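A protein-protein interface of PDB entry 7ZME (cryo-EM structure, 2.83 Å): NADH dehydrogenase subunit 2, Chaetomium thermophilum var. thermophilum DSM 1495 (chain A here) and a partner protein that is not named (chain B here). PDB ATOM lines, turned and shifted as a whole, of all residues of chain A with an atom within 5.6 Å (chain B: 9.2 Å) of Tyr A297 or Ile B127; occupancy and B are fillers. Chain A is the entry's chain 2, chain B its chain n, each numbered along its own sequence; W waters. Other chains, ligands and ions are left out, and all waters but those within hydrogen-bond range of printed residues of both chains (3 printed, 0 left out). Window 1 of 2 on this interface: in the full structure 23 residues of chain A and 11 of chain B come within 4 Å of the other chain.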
ATOM      1  N   LYS A  49     -17.649  12.697 -32.516  1.00  0.00           N
ATOM      2  CA  LYS A  49     -16.801  13.420 -31.584  1.00  0.00           C
ATOM      3  C   LYS A  49     -16.994  12.967 -30.147  1.00  0.00           C
ATOM      4  O   LYS A  49     -16.205  13.353 -29.280  1.00  0.00           O
ATOM      5  CB  LYS A  49     -17.068  14.923 -31.666  1.00  0.00           C
ATOM      6  CG  LYS A  49     -16.470  15.604 -32.866  1.00  0.00           C
ATOM      7  CD  LYS A  49     -16.378  17.094 -32.618  1.00  0.00           C
ATOM      8  CE  LYS A  49     -15.798  17.802 -33.809  1.00  0.00           C
ATOM      9  NZ  LYS A  49     -16.774  17.806 -34.918  1.00  0.00           N
ATOM     10  N   ASP A 207     -19.482  19.159 -20.771  1.00  0.00           N
ATOM     11  CA  ASP A 207     -20.254  19.502 -21.956  1.00  0.00           C
ATOM     12  C   ASP A 207     -20.970  20.835 -21.763  1.00  0.00           C
ATOM     13  O   ASP A 207     -20.986  21.679 -22.667  1.00  0.00           O
ATOM     14  CB  ASP A 207     -21.240  18.370 -22.241  1.00  0.00           C
ATOM     15  CG  ASP A 207     -21.945  18.510 -23.570  1.00  0.00           C
ATOM     16  OD1 ASP A 207     -21.707  19.501 -24.285  1.00  0.00           O
ATOM     17  OD2 ASP A 207     -22.742  17.608 -23.898  1.00  0.00           O
ATOM     18  N   TYR A 210     -18.276  23.589 -21.751  1.00  0.00           N
ATOM     19  CA  TYR A 210     -17.826  23.930 -23.095  1.00  0.00           C
ATOM     20  C   TYR A 210     -18.765  24.924 -23.760  1.00  0.00           C
ATOM     21  O   TYR A 210     -18.318  25.846 -24.450  1.00  0.00           O
ATOM     22  CB  TYR A 210     -17.704  22.666 -23.943  1.00  0.00           C
ATOM     23  CG  TYR A 210     -16.619  21.725 -23.489  1.00  0.00           C
ATOM     24  CD1 TYR A 210     -15.546  22.183 -22.739  1.00  0.00           C
ATOM     25  CD2 TYR A 210     -16.666  20.378 -23.808  1.00  0.00           C
ATOM     26  CE1 TYR A 210     -14.549  21.325 -22.318  1.00  0.00           C
ATOM     27  CE2 TYR A 210     -15.673  19.512 -23.394  1.00  0.00           C
ATOM     28  CZ  TYR A 210     -14.618  19.993 -22.649  1.00  0.00           C
ATOM     29  OH  TYR A 210     -13.625  19.142 -22.232  1.00  0.00           O
ATOM     30  N   ILE A 211     -20.074  24.747 -23.577  1.00  0.00           N
ATOM     31  CA  ILE A 211     -21.039  25.641 -24.208  1.00  0.00           C
ATOM     32  C   ILE A 211     -20.955  27.037 -23.605  1.00  0.00           C
ATOM     33  O   ILE A 211     -21.027  28.039 -24.324  1.00  0.00           O
ATOM     34  CB  ILE A 211     -22.456  25.052 -24.103  1.00  0.00           C
ATOM     35  CG1 ILE A 211     -22.624  23.920 -25.109  1.00  0.00           C
ATOM     36  CG2 ILE A 211     -23.506  26.116 -24.349  1.00  0.00           C
ATOM     37  CD1 ILE A 211     -24.026  23.422 -25.220  1.00  0.00           C
ATOM     38  N   ASN A 213     -18.277  28.418 -22.382  1.00  0.00           N
ATOM     39  CA  ASN A 213     -17.025  28.953 -22.977  1.00  0.00           C
ATOM     40  C   ASN A 213     -17.257  29.354 -24.432  1.00  0.00           C
ATOM     41  O   ASN A 213     -16.675  30.358 -24.866  1.00  0.00           O
ATOM     42  CB  ASN A 213     -15.889  27.931 -22.903  1.00  0.00           C
ATOM     43  CG  ASN A 213     -14.687  28.291 -23.750  1.00  0.00           C
ATOM     44  OD1 ASN A 213     -14.295  27.530 -24.629  1.00  0.00           O
ATOM     45  ND2 ASN A 213     -14.104  29.452 -23.505  1.00  0.00           N
ATOM     46  N   SER A 214     -18.094  28.621 -25.155  1.00  0.00           N
ATOM     47  CA  SER A 214     -18.258  28.885 -26.599  1.00  0.00           C
ATOM     48  C   SER A 214     -19.145  30.116 -26.785  1.00  0.00           C
ATOM     49  O   SER A 214     -18.750  31.002 -27.550  1.00  0.00           O
ATOM     50  CB  SER A 214     -18.846  27.697 -27.280  1.00  0.00           C
ATOM     51  OG  SER A 214     -18.989  27.926 -28.671  1.00  0.00           O
ATOM     52  N   LEU A 292      -5.966  16.540 -23.752  1.00  0.00           N
ATOM     53  CA  LEU A 292      -6.063  16.874 -25.191  1.00  0.00           C
ATOM     54  C   LEU A 292      -7.455  17.352 -25.571  1.00  0.00           C
ATOM     55  O   LEU A 292      -7.558  18.353 -26.295  1.00  0.00           O
ATOM     56  CB  LEU A 292      -5.731  15.628 -26.016  1.00  0.00           C
ATOM     57  CG  LEU A 292      -5.988  15.744 -27.517  1.00  0.00           C
ATOM     58  CD1 LEU A 292      -4.994  16.688 -28.172  1.00  0.00           C
ATOM     59  CD2 LEU A 292      -5.942  14.383 -28.183  1.00  0.00           C
ATOM     60  N   GLU A 293      -8.487  16.679 -25.086  1.00  0.00           N
ATOM     61  CA  GLU A 293      -9.831  17.056 -25.561  1.00  0.00           C
ATOM     62  C   GLU A 293     -10.293  18.271 -24.767  1.00  0.00           C
ATOM     63  O   GLU A 293     -11.102  19.047 -25.272  1.00  0.00           O
ATOM     64  CB  GLU A 293     -10.772  15.875 -25.393  1.00  0.00           C
ATOM     65  CG  GLU A 293     -11.868  15.819 -26.438  1.00  0.00           C
ATOM     66  CD  GLU A 293     -12.843  14.666 -26.274  1.00  0.00           C
ATOM     67  OE1 GLU A 293     -12.573  13.778 -25.446  1.00  0.00           O
ATOM     68  OE2 GLU A 293     -13.869  14.663 -26.978  1.00  0.00           O
ATOM     69  N   LEU A 294      -9.712  18.466 -23.591  1.00  0.00           N
ATOM     70  CA  LEU A 294     -10.099  19.643 -22.829  1.00  0.00           C
ATOM     71  C   LEU A 294      -9.391  20.890 -23.361  1.00  0.00           C
ATOM     72  O   LEU A 294      -9.919  22.000 -23.246  1.00  0.00           O
ATOM     73  CB  LEU A 294      -9.808  19.406 -21.345  1.00  0.00           C
ATOM     74  CG  LEU A 294     -10.283  20.381 -20.263  1.00  0.00           C
ATOM     75  CD1 LEU A 294     -10.445  19.617 -18.958  1.00  0.00           C
ATOM     76  CD2 LEU A 294      -9.415  21.581 -20.055  1.00  0.00           C
ATOM     77  N   VAL A 295      -8.196  20.723 -23.937  1.00  0.00           N
ATOM     78  CA  VAL A 295      -7.519  21.824 -24.619  1.00  0.00           C
ATOM     79  C   VAL A 295      -8.274  22.223 -25.881  1.00  0.00           C
ATOM     80  O   VAL A 295      -8.345  23.406 -26.230  1.00  0.00           O
ATOM     81  CB  VAL A 295      -6.058  21.440 -24.931  1.00  0.00           C
ATOM     82  CG1 VAL A 295      -5.426  22.449 -25.858  1.00  0.00           C
ATOM     83  CG2 VAL A 295      -5.245  21.352 -23.663  1.00  0.00           C
ATOM     84  N   TYR A 296      -8.811  21.259 -26.626  1.00  0.00           N
ATOM     85  CA  TYR A 296      -9.511  21.583 -27.895  1.00  0.00           C
ATOM     86  C   TYR A 296     -10.816  22.340 -27.660  1.00  0.00           C
ATOM     87  O   TYR A 296     -11.010  23.384 -28.295  1.00  0.00           O
ATOM     88  CB  TYR A 296      -9.872  20.308 -28.658  1.00  0.00           C
ATOM     89  CG  TYR A 296     -10.616  20.544 -29.948  1.00  0.00           C
ATOM     90  CD1 TYR A 296      -9.933  20.801 -31.123  1.00  0.00           C
ATOM     91  CD2 TYR A 296     -12.000  20.524 -29.998  1.00  0.00           C
ATOM     92  CE1 TYR A 296     -10.603  21.042 -32.309  1.00  0.00           C
ATOM     93  CE2 TYR A 296     -12.685  20.765 -31.176  1.00  0.00           C
ATOM     94  CZ  TYR A 296     -11.982  21.024 -32.337  1.00  0.00           C
ATOM     95  OH  TYR A 296     -12.640  21.254 -33.508  1.00  0.00           O
ATOM     96  N   TYR A 297     -11.678  21.858 -26.779  1.00  0.00           N
ATOM     97  CA  TYR A 297     -12.997  22.513 -26.609  1.00  0.00           C
ATOM     98  C   TYR A 297     -12.841  23.925 -26.028  1.00  0.00           C
ATOM     99  O   TYR A 297     -13.604  24.809 -26.433  1.00  0.00           O
ATOM    100  CB  TYR A 297     -14.007  21.559 -25.972  1.00  0.00           C
ATOM    101  CG  TYR A 297     -14.434  20.419 -26.856  1.00  0.00           C
ATOM    102  CD1 TYR A 297     -15.360  20.607 -27.866  1.00  0.00           C
ATOM    103  CD2 TYR A 297     -13.917  19.149 -26.681  1.00  0.00           C
ATOM    104  CE1 TYR A 297     -15.757  19.566 -28.686  1.00  0.00           C
ATOM    105  CE2 TYR A 297     -14.301  18.097 -27.492  1.00  0.00           C
ATOM    106  CZ  TYR A 297     -15.225  18.305 -28.498  1.00  0.00           C
ATOM    107  OH  TYR A 297     -15.603  17.264 -29.294  1.00  0.00           O
ATOM    108  N   THR A 298     -11.879  24.142 -25.134  1.00  0.00           N
ATOM    109  CA  THR A 298     -11.760  25.454 -24.449  1.00  0.00           C
ATOM    110  C   THR A 298     -10.943  26.468 -25.251  1.00  0.00           C
ATOM    111  O   THR A 298     -10.790  27.594 -24.753  1.00  0.00           O
ATOM    112  CB  THR A 298     -11.207  25.291 -23.030  1.00  0.00           C
ATOM    113  OG1 THR A 298      -9.911  24.705 -23.137  1.00  0.00           O
ATOM    114  CG2 THR A 298     -12.099  24.447 -22.146  1.00  0.00           C
ATOM    115  N   ASN A 299     -10.419  26.104 -26.423  1.00  0.00           N
ATOM    116  CA  ASN A 299      -9.709  27.116 -27.244  1.00  0.00           C
ATOM    117  C   ASN A 299     -10.704  28.146 -27.751  1.00  0.00           C
ATOM    118  O   ASN A 299     -11.772  27.736 -28.234  1.00  0.00           O
ATOM    119  CB  ASN A 299      -8.994  26.534 -28.459  1.00  0.00           C
ATOM    120  CG  ASN A 299      -7.487  26.628 -28.372  1.00  0.00           C
ATOM    121  OD1 ASN A 299      -6.920  26.606 -27.284  1.00  0.00           O
ATOM    122  ND2 ASN A 299      -6.833  26.723 -29.516  1.00  0.00           N
ATOM    123  N   LEU A 568     -11.895  14.919 -34.692  1.00  0.00           N
ATOM    124  CA  LEU A 568     -11.932  15.869 -33.584  1.00  0.00           C
ATOM    125  C   LEU A 568     -12.106  17.305 -34.067  1.00  0.00           C
ATOM    126  O   LEU A 568     -12.689  18.129 -33.354  1.00  0.00           O
ATOM    127  CB  LEU A 568     -10.660  15.740 -32.744  1.00  0.00           C
ATOM    128  CG  LEU A 568     -10.407  16.777 -31.643  1.00  0.00           C
ATOM    129  CD1 LEU A 568     -11.335  16.583 -30.458  1.00  0.00           C
ATOM    130  CD2 LEU A 568      -8.958  16.753 -31.202  1.00  0.00           C
ATOM    131  N   ARG B 123     -11.314  24.571 -38.367  1.00  0.00           N
ATOM    132  CA  ARG B 123     -11.646  24.034 -37.057  1.00  0.00           C
ATOM    133  C   ARG B 123     -13.055  24.451 -36.666  1.00  0.00           C
ATOM    134  O   ARG B 123     -13.419  25.626 -36.761  1.00  0.00           O
ATOM    135  CB  ARG B 123     -10.645  24.524 -36.014  1.00  0.00           C
ATOM    136  CG  ARG B 123     -11.047  24.246 -34.586  1.00  0.00           C
ATOM    137  CD  ARG B 123     -10.315  25.165 -33.641  1.00  0.00           C
ATOM    138  NE  ARG B 123     -10.346  24.680 -32.267  1.00  0.00           N
ATOM    139  CZ  ARG B 123      -9.271  24.305 -31.585  1.00  0.00           C
ATOM    140  NH1 ARG B 123      -8.077  24.354 -32.151  1.00  0.00           N
ATOM    141  NH2 ARG B 123      -9.393  23.878 -30.340  1.00  0.00           N
ATOM    142  N   SER B 124     -13.847  23.478 -36.230  1.00  0.00           N
ATOM    143  CA  SER B 124     -15.220  23.757 -35.844  1.00  0.00           C
ATOM    144  C   SER B 124     -15.266  24.513 -34.525  1.00  0.00           C
ATOM    145  O   SER B 124     -14.553  24.185 -33.574  1.00  0.00           O
ATOM    146  CB  SER B 124     -16.015  22.461 -35.725  1.00  0.00           C
ATOM    147  OG  SER B 124     -17.340  22.718 -35.297  1.00  0.00           O
ATOM    148  N   ARG B 125     -16.162  25.498 -34.460  1.00  0.00           N
ATOM    149  CA  ARG B 125     -16.340  26.273 -33.211  1.00  0.00           C
ATOM    150  C   ARG B 125     -17.726  25.979 -32.626  1.00  0.00           C
ATOM    151  O   ARG B 125     -18.122  26.680 -31.687  1.00  0.00           O
ATOM    152  CB  ARG B 125     -16.120  27.760 -33.499  1.00  0.00           C
ATOM    153  CG  ARG B 125     -16.840  28.266 -34.740  1.00  0.00           C
ATOM    154  CD  ARG B 125     -16.256  29.585 -35.205  1.00  0.00           C
ATOM    155  NE  ARG B 125     -14.887  29.441 -35.677  1.00  0.00           N
ATOM    156  CZ  ARG B 125     -14.148  30.438 -36.150  1.00  0.00           C
ATOM    157  NH1 ARG B 125     -14.649  31.659 -36.213  1.00  0.00           N
ATOM    158  NH2 ARG B 125     -12.912  30.210 -36.556  1.00  0.00           N
ATOM    159  N   HIS B 126     -18.439  25.000 -33.183  1.00  0.00           N
ATOM    160  CA  HIS B 126     -19.798  24.639 -32.696  1.00  0.00           C
ATOM    161  C   HIS B 126     -19.734  23.358 -31.866  1.00  0.00           C
ATOM    162  O   HIS B 126     -19.152  22.368 -32.348  1.00  0.00           O
ATOM    163  CB  HIS B 126     -20.789  24.540 -33.864  1.00  0.00           C
ATOM    164  CG  HIS B 126     -21.983  23.682 -33.616  1.00  0.00           C
ATOM    165  ND1 HIS B 126     -22.965  24.022 -32.715  1.00  0.00           N
ATOM    166  CD2 HIS B 126     -22.371  22.515 -34.173  1.00  0.00           C
ATOM    167  CE1 HIS B 126     -23.903  23.101 -32.717  1.00  0.00           C
ATOM    168  NE2 HIS B 126     -23.561  22.163 -33.600  1.00  0.00           N
ATOM    169  N   ILE B 127     -20.322  23.385 -30.670  1.00  0.00           N
ATOM    170  CA  ILE B 127     -20.347  22.185 -29.797  1.00  0.00           C
ATOM    171  C   ILE B 127     -21.651  21.433 -30.045  1.00  0.00           C
ATOM    172  O   ILE B 127     -22.707  22.059 -29.976  1.00  0.00           O
ATOM    173  CB  ILE B 127     -20.229  22.599 -28.317  1.00  0.00           C
ATOM    174  CG1 ILE B 127     -19.218  23.727 -28.097  1.00  0.00           C
ATOM    175  CG2 ILE B 127     -19.947  21.396 -27.430  1.00  0.00           C
ATOM    176  CD1 ILE B 127     -17.778  23.296 -28.195  1.00  0.00           C
ATOM    177  N   GLU B 128     -21.464  20.055 -30.358  1.00  0.00           N
ATOM    178  CA  GLU B 128     -22.652  19.166 -30.466  1.00  0.00           C
ATOM    179  C   GLU B 128     -22.689  18.385 -29.162  1.00  0.00           C
ATOM    180  O   GLU B 128     -21.674  17.771 -28.858  1.00  0.00           O
ATOM    181  CB  GLU B 128     -22.511  18.242 -31.675  1.00  0.00           C
ATOM    182  CG  GLU B 128     -23.687  17.326 -31.911  1.00  0.00           C
ATOM    183  CD  GLU B 128     -24.758  17.928 -32.797  1.00  0.00           C
ATOM    184  OE1 GLU B 128     -24.532  19.030 -33.330  1.00  0.00           O
ATOM    185  OE2 GLU B 128     -25.817  17.292 -32.947  1.00  0.00           O
ATOM    186  N   LEU B 129     -23.876  18.473 -28.399  1.00  0.00           N
ATOM    187  CA  LEU B 129     -23.883  17.764 -27.093  1.00  0.00           C
ATOM    188  C   LEU B 129     -23.608  16.277 -27.309  1.00  0.00           C
ATOM    189  O   LEU B 129     -24.293  15.675 -28.144  1.00  0.00           O
ATOM    190  CB  LEU B 129     -25.249  17.973 -26.437  1.00  0.00           C
ATOM    191  CG  LEU B 129     -25.684  19.421 -26.260  1.00  0.00           C
ATOM    192  CD1 LEU B 129     -27.075  19.491 -25.660  1.00  0.00           C
ATOM    193  CD2 LEU B 129     -24.694  20.148 -25.380  1.00  0.00           C
ATOM    194  N   LYS B 130     -22.626  15.716 -26.604  1.00  0.00           N
ATOM    195  CA  LYS B 130     -22.346  14.261 -26.650  1.00  0.00           C
ATOM    196  C   LYS B 130     -23.528  13.578 -25.989  1.00  0.00           C
ATOM    197  O   LYS B 130     -23.837  12.437 -26.356  1.00  0.00           O
ATOM    198  CB  LYS B 130     -21.104  13.928 -25.822  1.00  0.00           C
ATOM    199  CG  LYS B 130     -19.772  14.416 -26.368  1.00  0.00           C
ATOM    200  CD  LYS B 130     -18.636  14.221 -25.392  1.00  0.00           C
ATOM    201  CE  LYS B 130     -17.289  14.600 -25.969  1.00  0.00           C
ATOM    202  NZ  LYS B 130     -16.216  14.541 -24.950  1.00  0.00           N
ATOM    203  N   TYR B 131     -24.147  14.277 -25.031  1.00  0.00           N
ATOM    204  CA  TYR B 131     -25.315  13.751 -24.282  1.00  0.00           C
ATOM    205  C   TYR B 131     -26.509  14.707 -24.504  1.00  0.00           C
ATOM    206  O   TYR B 131     -26.757  15.532 -23.629  1.00  0.00           O
ATOM    207  CB  TYR B 131     -24.891  13.479 -22.842  1.00  0.00           C
ATOM    208  CG  TYR B 131     -25.942  12.919 -21.923  1.00  0.00           C
ATOM    209  CD1 TYR B 131     -26.433  11.637 -22.091  1.00  0.00           C
ATOM    210  CD2 TYR B 131     -26.403  13.659 -20.851  1.00  0.00           C
ATOM    211  CE1 TYR B 131     -27.384  11.114 -21.233  1.00  0.00           C
ATOM    212  CE2 TYR B 131     -27.347  13.150 -19.981  1.00  0.00           C
ATOM    213  CZ  TYR B 131     -27.844  11.877 -20.177  1.00  0.00           C
ATOM    214  OH  TYR B 131     -28.770  11.372 -19.319  1.00  0.00           O
ATOM    215  N   HIS B 157     -35.733  19.561 -33.576  1.00  0.00           N
ATOM    216  CA  HIS B 157     -34.329  19.551 -34.048  1.00  0.00           C
ATOM    217  C   HIS B 157     -33.788  18.128 -34.078  1.00  0.00           C
ATOM    218  O   HIS B 157     -33.301  17.698 -35.131  1.00  0.00           O
ATOM    219  CB  HIS B 157     -33.508  20.420 -33.095  1.00  0.00           C
ATOM    220  CG  HIS B 157     -32.071  20.572 -33.450  1.00  0.00           C
ATOM    221  ND1 HIS B 157     -31.612  21.630 -34.202  1.00  0.00           N
ATOM    222  CD2 HIS B 157     -30.993  19.821 -33.147  1.00  0.00           C
ATOM    223  CE1 HIS B 157     -30.311  21.518 -34.361  1.00  0.00           C
ATOM    224  NE2 HIS B 157     -29.909  20.420 -33.721  1.00  0.00           N
ATOM    225  N   TYR B 158     -33.779  17.474 -32.921  1.00  0.00           N
ATOM    226  CA  TYR B 158     -33.205  16.113 -32.801  1.00  0.00           C
ATOM    227  C   TYR B 158     -33.987  15.121 -33.660  1.00  0.00           C
ATOM    228  O   TYR B 158     -33.362  14.219 -34.227  1.00  0.00           O
ATOM    229  CB  TYR B 158     -33.035  15.753 -31.325  1.00  0.00           C
ATOM    230  CG  TYR B 158     -31.928  16.505 -30.637  1.00  0.00           C
ATOM    231  CD1 TYR B 158     -30.607  16.319 -31.005  1.00  0.00           C
ATOM    232  CD2 TYR B 158     -32.196  17.402 -29.618  1.00  0.00           C
ATOM    233  CE1 TYR B 158     -29.581  17.007 -30.383  1.00  0.00           C
ATOM    234  CE2 TYR B 158     -31.181  18.094 -28.980  1.00  0.00           C
ATOM    235  CZ  TYR B 158     -29.869  17.894 -29.364  1.00  0.00           C
ATOM    236  OH  TYR B 158     -28.863  18.567 -28.738  1.00  0.00           O
HETATM  237  O   HOH W   1     -18.653  17.045 -28.219  1.00  0.00           O
HETATM  238  O   HOH W   2     -24.937  17.171 -22.213  1.00  0.00           O
HETATM  239  O   HOH W   3     -20.503  17.569 -26.171  1.00  0.00           O
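OD2 of Asp A207 lies within hydrogen-bond range of N of Lys B130 (3.3 Å). The side-chain amino group (NZ) of Lys B130 is in salt-bridge range of the side-chain carboxylate (OE2) of Glu A293. The side-chain hydroxyl of Ser A214 sits at hydrogen-bond distance from the backbone carbonyl oxygen of Arg B125. The backbone carbonyl oxygen of Tyr A296 is in hydrogen-bond range of the guanidinium group of Arg B123, at 2.7 Å.
OH of Tyr A296 is in hydrogen-bond range of O of Leu A568. OD1 of Asn A213 lies close to O of Tyr A297 (3.3 Å). The backbone NH of His B126 sits at hydrogen-bond distance from the side-chain hydroxyl of Ser B124.
Among the printed residues, merely in contact across the chains: Lys A49 with Lys B130, Asp A207 with Leu B129, Asp A207 with Tyr B131, Ile A211 with Leu B129, Tyr A296 with Ser B124, Tyr A297 with Ile B127 and Asn A299 with Arg B123.
Printed residues of chain B within 4 Å of Lys A49: Lys B130. Of the printed residues of chain B, Ile A211 touches Leu B129 (3.3 Å). Of chain B, only Ile B127 comes within 4 Å of Tyr A297. No residue of chain B comes within 4 Å of Thr A298. Of chain A, only Tyr A297 comes within 4 Å of Ile B127. The nearest residue of chain B that does not touch Tyr A297 is Lys B130 (4.6 Å). The nearest printed residue of chain A that does not touch Ile B127 is Ser A214 (4.1 Å).
Printed residues of chain A that touch a printed residue of chain B: Lys A49, Asp A207, Ile A211, Ser A214, Glu A293, Tyr A296, Tyr A297 and Asn A299. Hydrophobic or aromatic side chains of chain A within 4 Å of the printed part of chain B: Ile A211, Tyr A296 and Tyr A297. Of the 11 printed residues of chain B, 7 touch a printed residue of chain A. Hydrophobic or aromatic side chains of chain B that line the printed part of chain A: Ile B127 and Leu B129. Among the printed residues, 11 pairs touch across the chains. Among the printed residues, Asp or Glu carboxylates within 4 Å of a Lys or Arg side-chain nitrogen of the other chain: Glu A293 with Lys B130 (3.1 Å).
Water W2 bridges OD2 of Asp A207 (2.8 Å) and O of Tyr B131 (2.8 Å). Water W3 lies within hydrogen-bond range of the backbone NH of Lys B130, the backbone carbonyl oxygen of Glu B128 and the side-chain carboxylate of Asp A207. Water W1 lies within hydrogen-bond range of O of Glu B128 (3.2 Å) and OH of Tyr A297 (3.2 Å).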
